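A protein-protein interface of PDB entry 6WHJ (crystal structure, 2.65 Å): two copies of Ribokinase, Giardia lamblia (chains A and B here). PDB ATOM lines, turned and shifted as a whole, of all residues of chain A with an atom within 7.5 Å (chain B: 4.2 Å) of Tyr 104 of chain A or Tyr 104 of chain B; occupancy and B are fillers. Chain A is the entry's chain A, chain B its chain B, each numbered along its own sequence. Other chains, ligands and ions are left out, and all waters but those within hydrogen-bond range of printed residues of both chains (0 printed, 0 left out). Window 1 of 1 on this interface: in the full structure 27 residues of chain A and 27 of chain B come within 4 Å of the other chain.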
ATOM      1  N   LEU A  19      20.565 -14.808 -40.251  1.00  0.00           N
ATOM      2  CA  LEU A  19      19.388 -15.158 -39.472  1.00  0.00           C
ATOM      3  C   LEU A  19      19.474 -14.347 -38.182  1.00  0.00           C
ATOM      4  O   LEU A  19      20.391 -14.551 -37.374  1.00  0.00           O
ATOM      5  CB  LEU A  19      19.371 -16.658 -39.198  1.00  0.00           C
ATOM      6  CG  LEU A  19      19.685 -17.536 -40.417  1.00  0.00           C
ATOM      7  CD1 LEU A  19      19.915 -18.965 -39.994  1.00  0.00           C
ATOM      8  CD2 LEU A  19      18.594 -17.470 -41.470  1.00  0.00           C
ATOM      9  N   VAL A  20      18.552 -13.402 -37.999  1.00  0.00           N
ATOM     10  CA  VAL A  20      18.717 -12.342 -37.009  1.00  0.00           C
ATOM     11  C   VAL A  20      17.528 -12.342 -36.054  1.00  0.00           C
ATOM     12  O   VAL A  20      16.373 -12.303 -36.490  1.00  0.00           O
ATOM     13  CB  VAL A  20      18.870 -10.967 -37.689  1.00  0.00           C
ATOM     14  CG1 VAL A  20      19.057  -9.867 -36.651  1.00  0.00           C
ATOM     15  CG2 VAL A  20      20.031 -10.977 -38.666  1.00  0.00           C
ATOM     16  N   TRP A  21      17.813 -12.321 -34.755  1.00  0.00           N
ATOM     17  CA  TRP A  21      16.799 -12.186 -33.720  1.00  0.00           C
ATOM     18  C   TRP A  21      16.999 -10.845 -33.031  1.00  0.00           C
ATOM     19  O   TRP A  21      18.111 -10.528 -32.596  1.00  0.00           O
ATOM     20  CB  TRP A  21      16.881 -13.328 -32.699  1.00  0.00           C
ATOM     21  CG  TRP A  21      16.417 -14.633 -33.241  1.00  0.00           C
ATOM     22  CD1 TRP A  21      15.176 -15.165 -33.115  1.00  0.00           C
ATOM     23  CD2 TRP A  21      17.177 -15.569 -34.023  1.00  0.00           C
ATOM     24  NE1 TRP A  21      15.109 -16.375 -33.757  1.00  0.00           N
ATOM     25  CE2 TRP A  21      16.321 -16.646 -34.327  1.00  0.00           C
ATOM     26  CE3 TRP A  21      18.495 -15.602 -34.491  1.00  0.00           C
ATOM     27  CZ2 TRP A  21      16.736 -17.745 -35.075  1.00  0.00           C
ATOM     28  CZ3 TRP A  21      18.907 -16.692 -35.240  1.00  0.00           C
ATOM     29  CH2 TRP A  21      18.030 -17.750 -35.525  1.00  0.00           C
ATOM     30  N   TYR A  22      15.923 -10.063 -32.937  1.00  0.00           N
ATOM     31  CA  TYR A  22      15.949  -8.734 -32.336  1.00  0.00           C
ATOM     32  C   TYR A  22      15.360  -8.820 -30.937  1.00  0.00           C
ATOM     33  O   TYR A  22      14.200  -9.209 -30.768  1.00  0.00           O
ATOM     34  CB  TYR A  22      15.183  -7.727 -33.188  1.00  0.00           C
ATOM     35  CG  TYR A  22      15.824  -7.501 -34.531  1.00  0.00           C
ATOM     36  CD1 TYR A  22      15.558  -8.347 -35.588  1.00  0.00           C
ATOM     37  CD2 TYR A  22      16.707  -6.449 -34.741  1.00  0.00           C
ATOM     38  CE1 TYR A  22      16.143  -8.155 -36.826  1.00  0.00           C
ATOM     39  CE2 TYR A  22      17.300  -6.245 -35.978  1.00  0.00           C
ATOM     40  CZ  TYR A  22      17.017  -7.106 -37.020  1.00  0.00           C
ATOM     41  OH  TYR A  22      17.589  -6.929 -38.268  1.00  0.00           O
ATOM     42  N   VAL A  23      16.171  -8.477 -29.940  1.00  0.00           N
ATOM     43  CA  VAL A  23      15.823  -8.648 -28.541  1.00  0.00           C
ATOM     44  C   VAL A  23      15.990  -7.316 -27.820  1.00  0.00           C
ATOM     45  O   VAL A  23      16.669  -6.402 -28.298  1.00  0.00           O
ATOM     46  CB  VAL A  23      16.707  -9.728 -27.882  1.00  0.00           C
ATOM     47  CG1 VAL A  23      16.521 -11.051 -28.591  1.00  0.00           C
ATOM     48  CG2 VAL A  23      18.164  -9.309 -27.920  1.00  0.00           C
ATOM     49  N   ASP A  25      17.404  -7.207 -24.650  1.00  0.00           N
ATOM     50  CA  ASP A  25      18.757  -7.354 -24.149  1.00  0.00           C
ATOM     51  C   ASP A  25      19.289  -8.721 -24.542  1.00  0.00           C
ATOM     52  O   ASP A  25      18.523  -9.673 -24.713  1.00  0.00           O
ATOM     53  CB  ASP A  25      18.814  -7.194 -22.628  1.00  0.00           C
ATOM     54  CG  ASP A  25      18.517  -5.777 -22.186  1.00  0.00           C
ATOM     55  OD1 ASP A  25      19.337  -4.871 -22.478  1.00  0.00           O
ATOM     56  OD2 ASP A  25      17.470  -5.580 -21.529  1.00  0.00           O
ATOM     57  N   PHE A  26      20.609  -8.809 -24.667  1.00  0.00           N
ATOM     58  CA  PHE A  26      21.228 -10.091 -24.930  1.00  0.00           C
ATOM     59  C   PHE A  26      20.817 -11.070 -23.836  1.00  0.00           C
ATOM     60  O   PHE A  26      20.755 -10.693 -22.658  1.00  0.00           O
ATOM     61  CB  PHE A  26      22.754  -9.974 -24.938  1.00  0.00           C
ATOM     62  CG  PHE A  26      23.305  -9.115 -26.031  1.00  0.00           C
ATOM     63  CD1 PHE A  26      22.943  -9.322 -27.352  1.00  0.00           C
ATOM     64  CD2 PHE A  26      24.213  -8.114 -25.738  1.00  0.00           C
ATOM     65  CE1 PHE A  26      23.458  -8.541 -28.353  1.00  0.00           C
ATOM     66  CE2 PHE A  26      24.736  -7.331 -26.737  1.00  0.00           C
ATOM     67  CZ  PHE A  26      24.359  -7.545 -28.045  1.00  0.00           C
ATOM     68  N   PRO A  27      20.509 -12.316 -24.178  1.00  0.00           N
ATOM     69  CA  PRO A  27      20.293 -13.312 -23.130  1.00  0.00           C
ATOM     70  C   PRO A  27      21.608 -13.556 -22.417  1.00  0.00           C
ATOM     71  O   PRO A  27      22.684 -13.358 -22.983  1.00  0.00           O
ATOM     72  CB  PRO A  27      19.833 -14.552 -23.901  1.00  0.00           C
ATOM     73  CG  PRO A  27      20.458 -14.385 -25.262  1.00  0.00           C
ATOM     74  CD  PRO A  27      20.424 -12.901 -25.531  1.00  0.00           C
ATOM     75  N   GLY A  30      22.476 -19.590 -20.185  1.00  0.00           N
ATOM     76  CA  GLY A  30      21.445 -20.396 -19.580  1.00  0.00           C
ATOM     77  C   GLY A  30      20.054 -19.819 -19.664  1.00  0.00           C
ATOM     78  O   GLY A  30      19.108 -20.473 -19.205  1.00  0.00           O
ATOM     79  N   GLN A  31      19.892 -18.625 -20.242  1.00  0.00           N
ATOM     80  CA  GLN A  31      18.615 -17.924 -20.274  1.00  0.00           C
ATOM     81  C   GLN A  31      17.877 -18.134 -21.596  1.00  0.00           C
ATOM     82  O   GLN A  31      18.484 -18.126 -22.671  1.00  0.00           O
ATOM     83  CB  GLN A  31      18.819 -16.423 -20.032  1.00  0.00           C
ATOM     84  CG  GLN A  31      17.552 -15.676 -19.631  1.00  0.00           C
ATOM     85  CD  GLN A  31      17.742 -14.166 -19.570  1.00  0.00           C
ATOM     86  OE1 GLN A  31      18.720 -13.618 -20.093  1.00  0.00           O
ATOM     87  NE2 GLN A  31      16.795 -13.481 -18.933  1.00  0.00           N
ATOM     88  N   ILE A  33      14.982 -16.243 -23.704  1.00  0.00           N
ATOM     89  CA  ILE A  33      14.205 -15.028 -23.878  1.00  0.00           C
ATOM     90  C   ILE A  33      13.507 -15.094 -25.229  1.00  0.00           C
ATOM     91  O   ILE A  33      13.788 -15.962 -26.061  1.00  0.00           O
ATOM     92  CB  ILE A  33      15.063 -13.756 -23.766  1.00  0.00           C
ATOM     93  CG1 ILE A  33      16.036 -13.660 -24.946  1.00  0.00           C
ATOM     94  CG2 ILE A  33      15.789 -13.728 -22.424  1.00  0.00           C
ATOM     95  CD1 ILE A  33      16.884 -12.433 -24.918  1.00  0.00           C
ATOM     96  N   ALA A 101      24.892 -16.921 -40.658  1.00  0.00           N
ATOM     97  CA  ALA A 101      25.261 -16.281 -39.406  1.00  0.00           C
ATOM     98  C   ALA A 101      24.054 -16.243 -38.487  1.00  0.00           C
ATOM     99  O   ALA A 101      22.955 -15.874 -38.907  1.00  0.00           O
ATOM    100  CB  ALA A 101      25.784 -14.855 -39.635  1.00  0.00           C
ATOM    101  N   GLY A 102      24.267 -16.615 -37.220  1.00  0.00           N
ATOM    102  CA  GLY A 102      23.254 -16.477 -36.201  1.00  0.00           C
ATOM    103  C   GLY A 102      23.552 -15.232 -35.393  1.00  0.00           C
ATOM    104  O   GLY A 102      24.574 -15.155 -34.714  1.00  0.00           O
ATOM    105  N   ILE A 103      22.646 -14.262 -35.461  1.00  0.00           N
ATOM    106  CA  ILE A 103      22.902 -12.906 -34.988  1.00  0.00           C
ATOM    107  C   ILE A 103      21.856 -12.538 -33.941  1.00  0.00           C
ATOM    108  O   ILE A 103      20.662 -12.814 -34.126  1.00  0.00           O
ATOM    109  CB  ILE A 103      22.881 -11.902 -36.158  1.00  0.00           C
ATOM    110  CG1 ILE A 103      23.887 -12.311 -37.236  1.00  0.00           C
ATOM    111  CG2 ILE A 103      23.151 -10.490 -35.666  1.00  0.00           C
ATOM    112  CD1 ILE A 103      23.910 -11.392 -38.434  1.00  0.00           C
ATOM    113  N   TYR A 104      22.311 -11.956 -32.826  1.00  0.00           N
ATOM    114  CA  TYR A 104      21.453 -11.289 -31.850  1.00  0.00           C
ATOM    115  C   TYR A 104      21.682  -9.783 -31.919  1.00  0.00           C
ATOM    116  O   TYR A 104      22.815  -9.325 -31.754  1.00  0.00           O
ATOM    117  CB  TYR A 104      21.738 -11.749 -30.419  1.00  0.00           C
ATOM    118  CG  TYR A 104      21.522 -13.212 -30.095  1.00  0.00           C
ATOM    119  CD1 TYR A 104      20.759 -14.039 -30.910  1.00  0.00           C
ATOM    120  CD2 TYR A 104      22.090 -13.759 -28.957  1.00  0.00           C
ATOM    121  CE1 TYR A 104      20.568 -15.375 -30.589  1.00  0.00           C
ATOM    122  CE2 TYR A 104      21.908 -15.081 -28.630  1.00  0.00           C
ATOM    123  CZ  TYR A 104      21.150 -15.886 -29.444  1.00  0.00           C
ATOM    124  OH  TYR A 104      20.980 -17.201 -29.088  1.00  0.00           O
ATOM    125  N   VAL A 105      20.611  -9.015 -32.107  1.00  0.00           N
ATOM    126  CA  VAL A 105      20.678  -7.557 -32.119  1.00  0.00           C
ATOM    127  C   VAL A 105      19.888  -7.029 -30.928  1.00  0.00           C
ATOM    128  O   VAL A 105      18.663  -7.201 -30.860  1.00  0.00           O
ATOM    129  CB  VAL A 105      20.158  -6.973 -33.440  1.00  0.00           C
ATOM    130  CG1 VAL A 105      20.268  -5.466 -33.432  1.00  0.00           C
ATOM    131  CG2 VAL A 105      20.961  -7.530 -34.604  1.00  0.00           C
ATOM    132  N   ALA A 106      20.589  -6.393 -29.985  1.00  0.00           N
ATOM    133  CA  ALA A 106      19.962  -5.773 -28.824  1.00  0.00           C
ATOM    134  C   ALA A 106      19.427  -4.388 -29.189  1.00  0.00           C
ATOM    135  O   ALA A 106      19.851  -3.773 -30.173  1.00  0.00           O
ATOM    136  CB  ALA A 106      20.952  -5.674 -27.662  1.00  0.00           C
ATOM    137  N   GLY A 109      21.634  -1.524 -30.210  1.00  0.00           N
ATOM    138  CA  GLY A 109      22.359  -1.577 -31.461  1.00  0.00           C
ATOM    139  C   GLY A 109      23.520  -2.551 -31.458  1.00  0.00           C
ATOM    140  O   GLY A 109      24.090  -2.822 -32.520  1.00  0.00           O
ATOM    141  N   GLU A 110      23.876  -3.086 -30.293  1.00  0.00           N
ATOM    142  CA  GLU A 110      24.981  -4.021 -30.193  1.00  0.00           C
ATOM    143  C   GLU A 110      24.624  -5.350 -30.862  1.00  0.00           C
ATOM    144  O   GLU A 110      23.454  -5.735 -30.941  1.00  0.00           O
ATOM    145  CB  GLU A 110      25.334  -4.229 -28.717  1.00  0.00           C
ATOM    146  CG  GLU A 110      26.754  -4.675 -28.466  1.00  0.00           C
ATOM    147  CD  GLU A 110      27.355  -3.997 -27.252  1.00  0.00           C
ATOM    148  OE1 GLU A 110      26.813  -4.177 -26.137  1.00  0.00           O
ATOM    149  OE2 GLU A 110      28.357  -3.265 -27.415  1.00  0.00           O
ATOM    150  N   ASN A 111      25.650  -6.047 -31.353  1.00  0.00           N
ATOM    151  CA  ASN A 111      25.498  -7.309 -32.063  1.00  0.00           C
ATOM    152  C   ASN A 111      26.220  -8.439 -31.346  1.00  0.00           C
ATOM    153  O   ASN A 111      27.174  -8.232 -30.595  1.00  0.00           O
ATOM    154  CB  ASN A 111      26.078  -7.246 -33.479  1.00  0.00           C
ATOM    155  CG  ASN A 111      25.276  -6.381 -34.402  1.00  0.00           C
ATOM    156  OD1 ASN A 111      24.176  -5.937 -34.067  1.00  0.00           O
ATOM    157  ND2 ASN A 111      25.835  -6.108 -35.575  1.00  0.00           N
ATOM    158  N   MET A 112      25.750  -9.650 -31.614  1.00  0.00           N
ATOM    159  CA  MET A 112      26.479 -10.880 -31.365  1.00  0.00           C
ATOM    160  C   MET A 112      26.372 -11.652 -32.665  1.00  0.00           C
ATOM    161  O   MET A 112      25.264 -11.816 -33.182  1.00  0.00           O
ATOM    162  CB  MET A 112      25.874 -11.692 -30.211  1.00  0.00           C
ATOM    163  CG  MET A 112      26.086 -11.124 -28.833  1.00  0.00           C
ATOM    164  SD  MET A 112      25.133 -12.087 -27.653  1.00  0.00           S
ATOM    165  CE  MET A 112      26.190 -12.034 -26.218  1.00  0.00           C
ATOM    166  N   ILE A 113      27.500 -12.074 -33.227  1.00  0.00           N
ATOM    167  CA  ILE A 113      27.495 -12.742 -34.523  1.00  0.00           C
ATOM    168  C   ILE A 113      28.256 -14.050 -34.410  1.00  0.00           C
ATOM    169  O   ILE A 113      29.417 -14.067 -33.989  1.00  0.00           O
ATOM    170  CB  ILE A 113      28.087 -11.855 -35.643  1.00  0.00           C
ATOM    171  CG1 ILE A 113      27.314 -10.541 -35.751  1.00  0.00           C
ATOM    172  CG2 ILE A 113      28.078 -12.573 -36.991  1.00  0.00           C
ATOM    173  CD1 ILE A 113      27.790  -9.653 -36.851  1.00  0.00           C
ATOM    174  N   VAL A 114      27.609 -15.135 -34.812  1.00  0.00           N
ATOM    175  CA  VAL A 114      28.232 -16.441 -34.958  1.00  0.00           C
ATOM    176  C   VAL A 114      28.075 -16.845 -36.412  1.00  0.00           C
ATOM    177  O   VAL A 114      26.950 -16.929 -36.915  1.00  0.00           O
ATOM    178  CB  VAL A 114      27.596 -17.480 -34.022  1.00  0.00           C
ATOM    179  CG1 VAL A 114      28.237 -18.825 -34.224  1.00  0.00           C
ATOM    180  CG2 VAL A 114      27.734 -17.035 -32.579  1.00  0.00           C
ATOM    181  N   ILE A 115      29.189 -17.052 -37.095  1.00  0.00           N
ATOM    182  CA  ILE A 115      29.187 -17.449 -38.500  1.00  0.00           C
ATOM    183  C   ILE A 115      29.444 -18.945 -38.590  1.00  0.00           C
ATOM    184  O   ILE A 115      30.317 -19.479 -37.893  1.00  0.00           O
ATOM    185  CB  ILE A 115      30.244 -16.669 -39.316  1.00  0.00           C
ATOM    186  CG1 ILE A 115      30.044 -15.164 -39.180  1.00  0.00           C
ATOM    187  CG2 ILE A 115      30.199 -17.067 -40.786  1.00  0.00           C
ATOM    188  CD1 ILE A 115      31.033 -14.362 -39.958  1.00  0.00           C
ATOM    189  N   TRP B  21      23.878 -22.927 -33.202  1.00  0.00           N
ATOM    190  CA  TRP B  21      25.290 -22.759 -33.524  1.00  0.00           C
ATOM    191  C   TRP B  21      26.134 -23.234 -32.349  1.00  0.00           C
ATOM    192  O   TRP B  21      25.909 -22.818 -31.206  1.00  0.00           O
ATOM    193  CB  TRP B  21      25.621 -21.298 -33.861  1.00  0.00           C
ATOM    194  CG  TRP B  21      25.080 -20.823 -35.186  1.00  0.00           C
ATOM    195  CD1 TRP B  21      25.751 -20.763 -36.373  1.00  0.00           C
ATOM    196  CD2 TRP B  21      23.757 -20.350 -35.449  1.00  0.00           C
ATOM    197  NE1 TRP B  21      24.930 -20.276 -37.357  1.00  0.00           N
ATOM    198  CE2 TRP B  21      23.699 -20.016 -36.819  1.00  0.00           C
ATOM    199  CE3 TRP B  21      22.613 -20.178 -34.661  1.00  0.00           C
ATOM    200  CZ2 TRP B  21      22.540 -19.530 -37.419  1.00  0.00           C
ATOM    201  CZ3 TRP B  21      21.465 -19.684 -35.259  1.00  0.00           C
ATOM    202  CH2 TRP B  21      21.439 -19.367 -36.623  1.00  0.00           C
ATOM    203  N   PHE B  26      30.365 -18.376 -25.705  1.00  0.00           N
ATOM    204  CA  PHE B  26      29.408 -17.394 -26.178  1.00  0.00           C
ATOM    205  C   PHE B  26      30.163 -16.159 -26.652  1.00  0.00           C
ATOM    206  O   PHE B  26      31.147 -15.749 -26.023  1.00  0.00           O
ATOM    207  CB  PHE B  26      28.430 -16.997 -25.076  1.00  0.00           C
ATOM    208  CG  PHE B  26      27.568 -18.116 -24.593  1.00  0.00           C
ATOM    209  CD1 PHE B  26      26.845 -18.889 -25.486  1.00  0.00           C
ATOM    210  CD2 PHE B  26      27.467 -18.384 -23.238  1.00  0.00           C
ATOM    211  CE1 PHE B  26      26.036 -19.924 -25.033  1.00  0.00           C
ATOM    212  CE2 PHE B  26      26.664 -19.413 -22.779  1.00  0.00           C
ATOM    213  CZ  PHE B  26      25.946 -20.185 -23.680  1.00  0.00           C
ATOM    214  N   PRO B  27      29.762 -15.561 -27.764  1.00  0.00           N
ATOM    215  CA  PRO B  27      30.361 -14.287 -28.156  1.00  0.00           C
ATOM    216  C   PRO B  27      29.966 -13.218 -27.154  1.00  0.00           C
ATOM    217  O   PRO B  27      28.918 -13.297 -26.513  1.00  0.00           O
ATOM    218  CB  PRO B  27      29.746 -14.018 -29.532  1.00  0.00           C
ATOM    219  CG  PRO B  27      28.422 -14.725 -29.465  1.00  0.00           C
ATOM    220  CD  PRO B  27      28.661 -15.960 -28.658  1.00  0.00           C
ATOM    221  N   GLY B 102      16.919 -19.222 -32.068  1.00  0.00           N
ATOM    222  CA  GLY B 102      18.323 -19.062 -32.378  1.00  0.00           C
ATOM    223  C   GLY B 102      19.134 -19.375 -31.139  1.00  0.00           C
ATOM    224  O   GLY B 102      19.041 -18.673 -30.132  1.00  0.00           O
ATOM    225  N   ILE B 103      19.939 -20.430 -31.222  1.00  0.00           N
ATOM    226  CA  ILE B 103      20.558 -21.033 -30.050  1.00  0.00           C
ATOM    227  C   ILE B 103      22.071 -21.025 -30.213  1.00  0.00           C
ATOM    228  O   ILE B 103      22.590 -21.398 -31.271  1.00  0.00           O
ATOM    229  CB  ILE B 103      20.027 -22.462 -29.818  1.00  0.00           C
ATOM    230  CG1 ILE B 103      18.504 -22.429 -29.634  1.00  0.00           C
ATOM    231  CG2 ILE B 103      20.725 -23.120 -28.631  1.00  0.00           C
ATOM    232  CD1 ILE B 103      17.870 -23.778 -29.417  1.00  0.00           C
ATOM    233  N   TYR B 104      22.769 -20.580 -29.169  1.00  0.00           N
ATOM    234  CA  TYR B 104      24.211 -20.742 -29.028  1.00  0.00           C
ATOM    235  C   TYR B 104      24.497 -21.782 -27.951  1.00  0.00           C
ATOM    236  O   TYR B 104      23.993 -21.677 -26.825  1.00  0.00           O
ATOM    237  CB  TYR B 104      24.908 -19.436 -28.640  1.00  0.00           C
ATOM    238  CG  TYR B 104      24.788 -18.278 -29.602  1.00  0.00           C
ATOM    239  CD1 TYR B 104      24.388 -18.459 -30.922  1.00  0.00           C
ATOM    240  CD2 TYR B 104      25.105 -16.992 -29.182  1.00  0.00           C
ATOM    241  CE1 TYR B 104      24.298 -17.377 -31.792  1.00  0.00           C
ATOM    242  CE2 TYR B 104      25.018 -15.919 -30.029  1.00  0.00           C
ATOM    243  CZ  TYR B 104      24.619 -16.111 -31.329  1.00  0.00           C
ATOM    244  OH  TYR B 104      24.540 -15.013 -32.148  1.00  0.00           O
ATOM    245  N   VAL B 105      25.301 -22.782 -28.293  1.00  0.00           N
ATOM    246  CA  VAL B 105      25.732 -23.798 -27.347  1.00  0.00           C
ATOM    247  C   VAL B 105      27.241 -23.671 -27.187  1.00  0.00           C
ATOM    248  O   VAL B 105      27.989 -23.825 -28.164  1.00  0.00           O
ATOM    249  CB  VAL B 105      25.329 -25.205 -27.806  1.00  0.00           C
ATOM    250  CG1 VAL B 105      25.686 -26.223 -26.753  1.00  0.00           C
ATOM    251  CG2 VAL B 105      23.837 -25.245 -28.100  1.00  0.00           C
ATOM    252  N   ALA B 106      27.683 -23.337 -25.972  1.00  0.00           N
ATOM    253  CA  ALA B 106      29.105 -23.270 -25.671  1.00  0.00           C
ATOM    254  C   ALA B 106      29.642 -24.670 -25.388  1.00  0.00           C
ATOM    255  O   ALA B 106      28.882 -25.623 -25.187  1.00  0.00           O
ATOM    256  CB  ALA B 106      29.370 -22.346 -24.483  1.00  0.00           C
ATOM    257  N   GLU B 110      26.380 -24.914 -21.872  1.00  0.00           N
ATOM    258  CA  GLU B 110      25.434 -23.849 -21.593  1.00  0.00           C
ATOM    259  C   GLU B 110      24.780 -23.365 -22.887  1.00  0.00           C
ATOM    260  O   GLU B 110      25.340 -23.488 -23.978  1.00  0.00           O
ATOM    261  CB  GLU B 110      26.148 -22.696 -20.881  1.00  0.00           C
ATOM    262  CG  GLU B 110      25.238 -21.870 -19.984  1.00  0.00           C
ATOM    263  CD  GLU B 110      25.984 -20.962 -19.007  1.00  0.00           C
ATOM    264  OE1 GLU B 110      27.172 -20.609 -19.247  1.00  0.00           O
ATOM    265  OE2 GLU B 110      25.363 -20.600 -17.982  1.00  0.00           O
ATOM    266  N   ASN B 111      23.572 -22.826 -22.756  1.00  0.00           N
ATOM    267  CA  ASN B 111      22.781 -22.366 -23.884  1.00  0.00           C
ATOM    268  C   ASN B 111      22.511 -20.873 -23.790  1.00  0.00           C
ATOM    269  O   ASN B 111      22.538 -20.276 -22.712  1.00  0.00           O
ATOM    270  CB  ASN B 111      21.415 -23.080 -23.944  1.00  0.00           C
ATOM    271  CG  ASN B 111      21.520 -24.533 -24.351  1.00  0.00           C
ATOM    272  OD1 ASN B 111      22.584 -25.010 -24.754  1.00  0.00           O
ATOM    273  ND2 ASN B 111      20.408 -25.251 -24.244  1.00  0.00           N
ATOM    274  N   MET B 112      22.242 -20.284 -24.949  1.00  0.00           N
ATOM    275  CA  MET B 112      21.541 -19.017 -25.059  1.00  0.00           C
ATOM    276  C   MET B 112      20.429 -19.286 -26.054  1.00  0.00           C
ATOM    277  O   MET B 112      20.695 -19.800 -27.143  1.00  0.00           O
ATOM    278  CB  MET B 112      22.427 -17.871 -25.557  1.00  0.00           C
ATOM    279  CG  MET B 112      23.451 -17.369 -24.568  1.00  0.00           C
ATOM    280  SD  MET B 112      24.509 -16.115 -25.301  1.00  0.00           S
ATOM    281  CE  MET B 112      24.932 -15.120 -23.876  1.00  0.00           C
ATOM    282  N   VAL B 114      16.966 -17.652 -27.945  1.00  0.00           N
ATOM    283  CA  VAL B 114      16.034 -16.588 -28.290  1.00  0.00           C
ATOM    284  C   VAL B 114      14.943 -17.208 -29.150  1.00  0.00           C
ATOM    285  O   VAL B 114      15.228 -17.762 -30.220  1.00  0.00           O
ATOM    286  CB  VAL B 114      16.711 -15.429 -29.035  1.00  0.00           C
ATOM    287  CG1 VAL B 114      15.671 -14.362 -29.352  1.00  0.00           C
ATOM    288  CG2 VAL B 114      17.833 -14.849 -28.224  1.00  0.00           C
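Of chain B, only Gly 102, Ile 103, Tyr 104, Met 112 and Val 114 come within 4 Å of Tyr 104 of chain A.
Of the printed residues of chain B, Ile 33 of chain A touches Val 114.
Of the printed residues of chain A, Glu 110 of chain B touches Gly 30 (3.6 Å).
Printed residues of chain B within 4 Å of Val 114 of chain A: Trp 21 (3.6 Å), Pro 27 (3.9 Å) and Tyr 104 (3.5 Å).
Of the printed residues of chain A, Val 114 of chain B touches Trp 21, Val 23, Pro 27, Ile 33 and Tyr 104.
Printed residues of chain B within 4 Å of Ile 103 of chain A: Tyr 104 (3.9 Å).
Gly 109 of chain A touches none of the printed residues of chain B.
Phe 26 of chain A touches none of the printed residues of chain B.
The nearest printed residue of chain B that does not touch Tyr 104 of chain A is Trp 21 of chain B (6.4 Å).
The nearest residue of chain A that does not touch Tyr 104 of chain B is Ile 113 of chain A (4.3 Å).
Trp 21 of chain A touches its own counterpart, Trp 21 of chain B.
Trp 21 of chain A touches Gly 102 of chain B, and with the chains exchanged Gly 102 of chain A touches Trp 21 of chain B.
Gly 102 of chain A touches Tyr 104 of chain B, and with the chains exchanged Tyr 104 of chain A touches Gly 102 of chain B.
Tyr 104 of chain A touches its own counterpart, Tyr 104 of chain B.
Of the 26 pairs that touch across the chains among the printed residues, 18 have their exchanged pair printed and touching as well.
Among the printed residues, merely in contact across the chains: Leu 19 of chain A with Trp 21 of chain B (3.7 Å), Trp 21 of chain A with Trp 21 of chain B (3.9 Å), Trp 21 of chain A with Gly 102 of chain B (3.4 Å), Trp 21 of chain A with Val 114 of chain B (3.7 Å), Val 23 of chain A with Val 114 of chain B (3.5 Å), Pro 27 of chain A with Met 112 of chain B (3.0 Å), Pro 27 of chain A with Val 114 of chain B (3.98 Å), Gly 30 of chain A with Glu 110 of chain B (3.6 Å), Gln 31 of chain A with Asn 111 of chain B (3.98 Å), Gln 31 of chain A with Met 112 of chain B (3.98 Å), Ile 33 of chain A with Val 114 of chain B (3.2 Å), Ala 101 of chain A with Trp 21 of chain B (3.8 Å), Gly 102 of chain A with Trp 21 of chain B (3.4 Å), Ile 103 of chain A with Tyr 104 of chain B (3.9 Å), Tyr 104 of chain A with Ile 103 of chain B (3.97 Å), Tyr 104 of chain A with Tyr 104 of chain B (3.5 Å), Tyr 104 of chain A with Val 114 of chain B (3.7 Å), Met 112 of chain A with Pro 27 of chain B (3.0 Å), Val 114 of chain A with Trp 21 of chain B (3.6 Å), Val 114 of chain A with Pro 27 of chain B (3.9 Å) and Val 114 of chain A with Tyr 104 of chain B (3.5 Å).
O of Ala 101 of chain A is in hydrogen-bond range of N of Leu 19 of chain A, at 2.9 Å.
The backbone carbonyl oxygen (O) of Leu 19 of chain A lies within hydrogen-bond range of the backbone NH (N) of Ile 103 of chain A (3.0 Å).
The backbone carbonyl oxygen (O) of Ile 103 of chain A lies within hydrogen-bond range of the backbone NH (N) of Trp 21 of chain A.
O of Trp 21 of chain A lies within hydrogen-bond range of N of Val 105 of chain A, 3.0 Å away.
O of Tyr 104 of chain A sits at hydrogen-bond distance from N of Met 112 of chain A (3.0 Å).
N of Val 105 of chain B sits at hydrogen-bond distance from O of Trp 21 of chain B, at 3.0 Å.
Printed residues of chain A that touch a printed residue of chain B: Leu 19, Trp 21, Val 23, Pro 27, Gly 30, Gln 31, Ile 33, Ala 101, Gly 102, Ile 103, Tyr 104, Met 112 and Val 114.
Hydrophobic or aromatic side chains of chain A that line the printed part of chain B: Leu 19, Trp 21, Val 23, Pro 27, Ile 33, Tyr 104, Met 112 and Val 114.
N of Gly 30 of chain A lies within hydrogen-bond range of O of Asn 111 of chain B (2.6 Å).
O of Gly 102 of chain A is in hydrogen-bond range of OH of Tyr 104 of chain B, 2.6 Å away.
The side-chain hydroxyl (OH) of Tyr 104 of chain A is in hydrogen-bond range of the backbone carbonyl oxygen (O) of Gly 102 of chain B (2.6 Å).
The backbone carbonyl oxygen (O) of Met 112 of chain B lies within hydrogen-bond range of the side-chain hydroxyl (OH) of Tyr 104 of chain A (3.3 Å).
OH of Tyr 104 of chain B sits at hydrogen-bond distance from O of Met 112 of chain A (3.4 Å).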
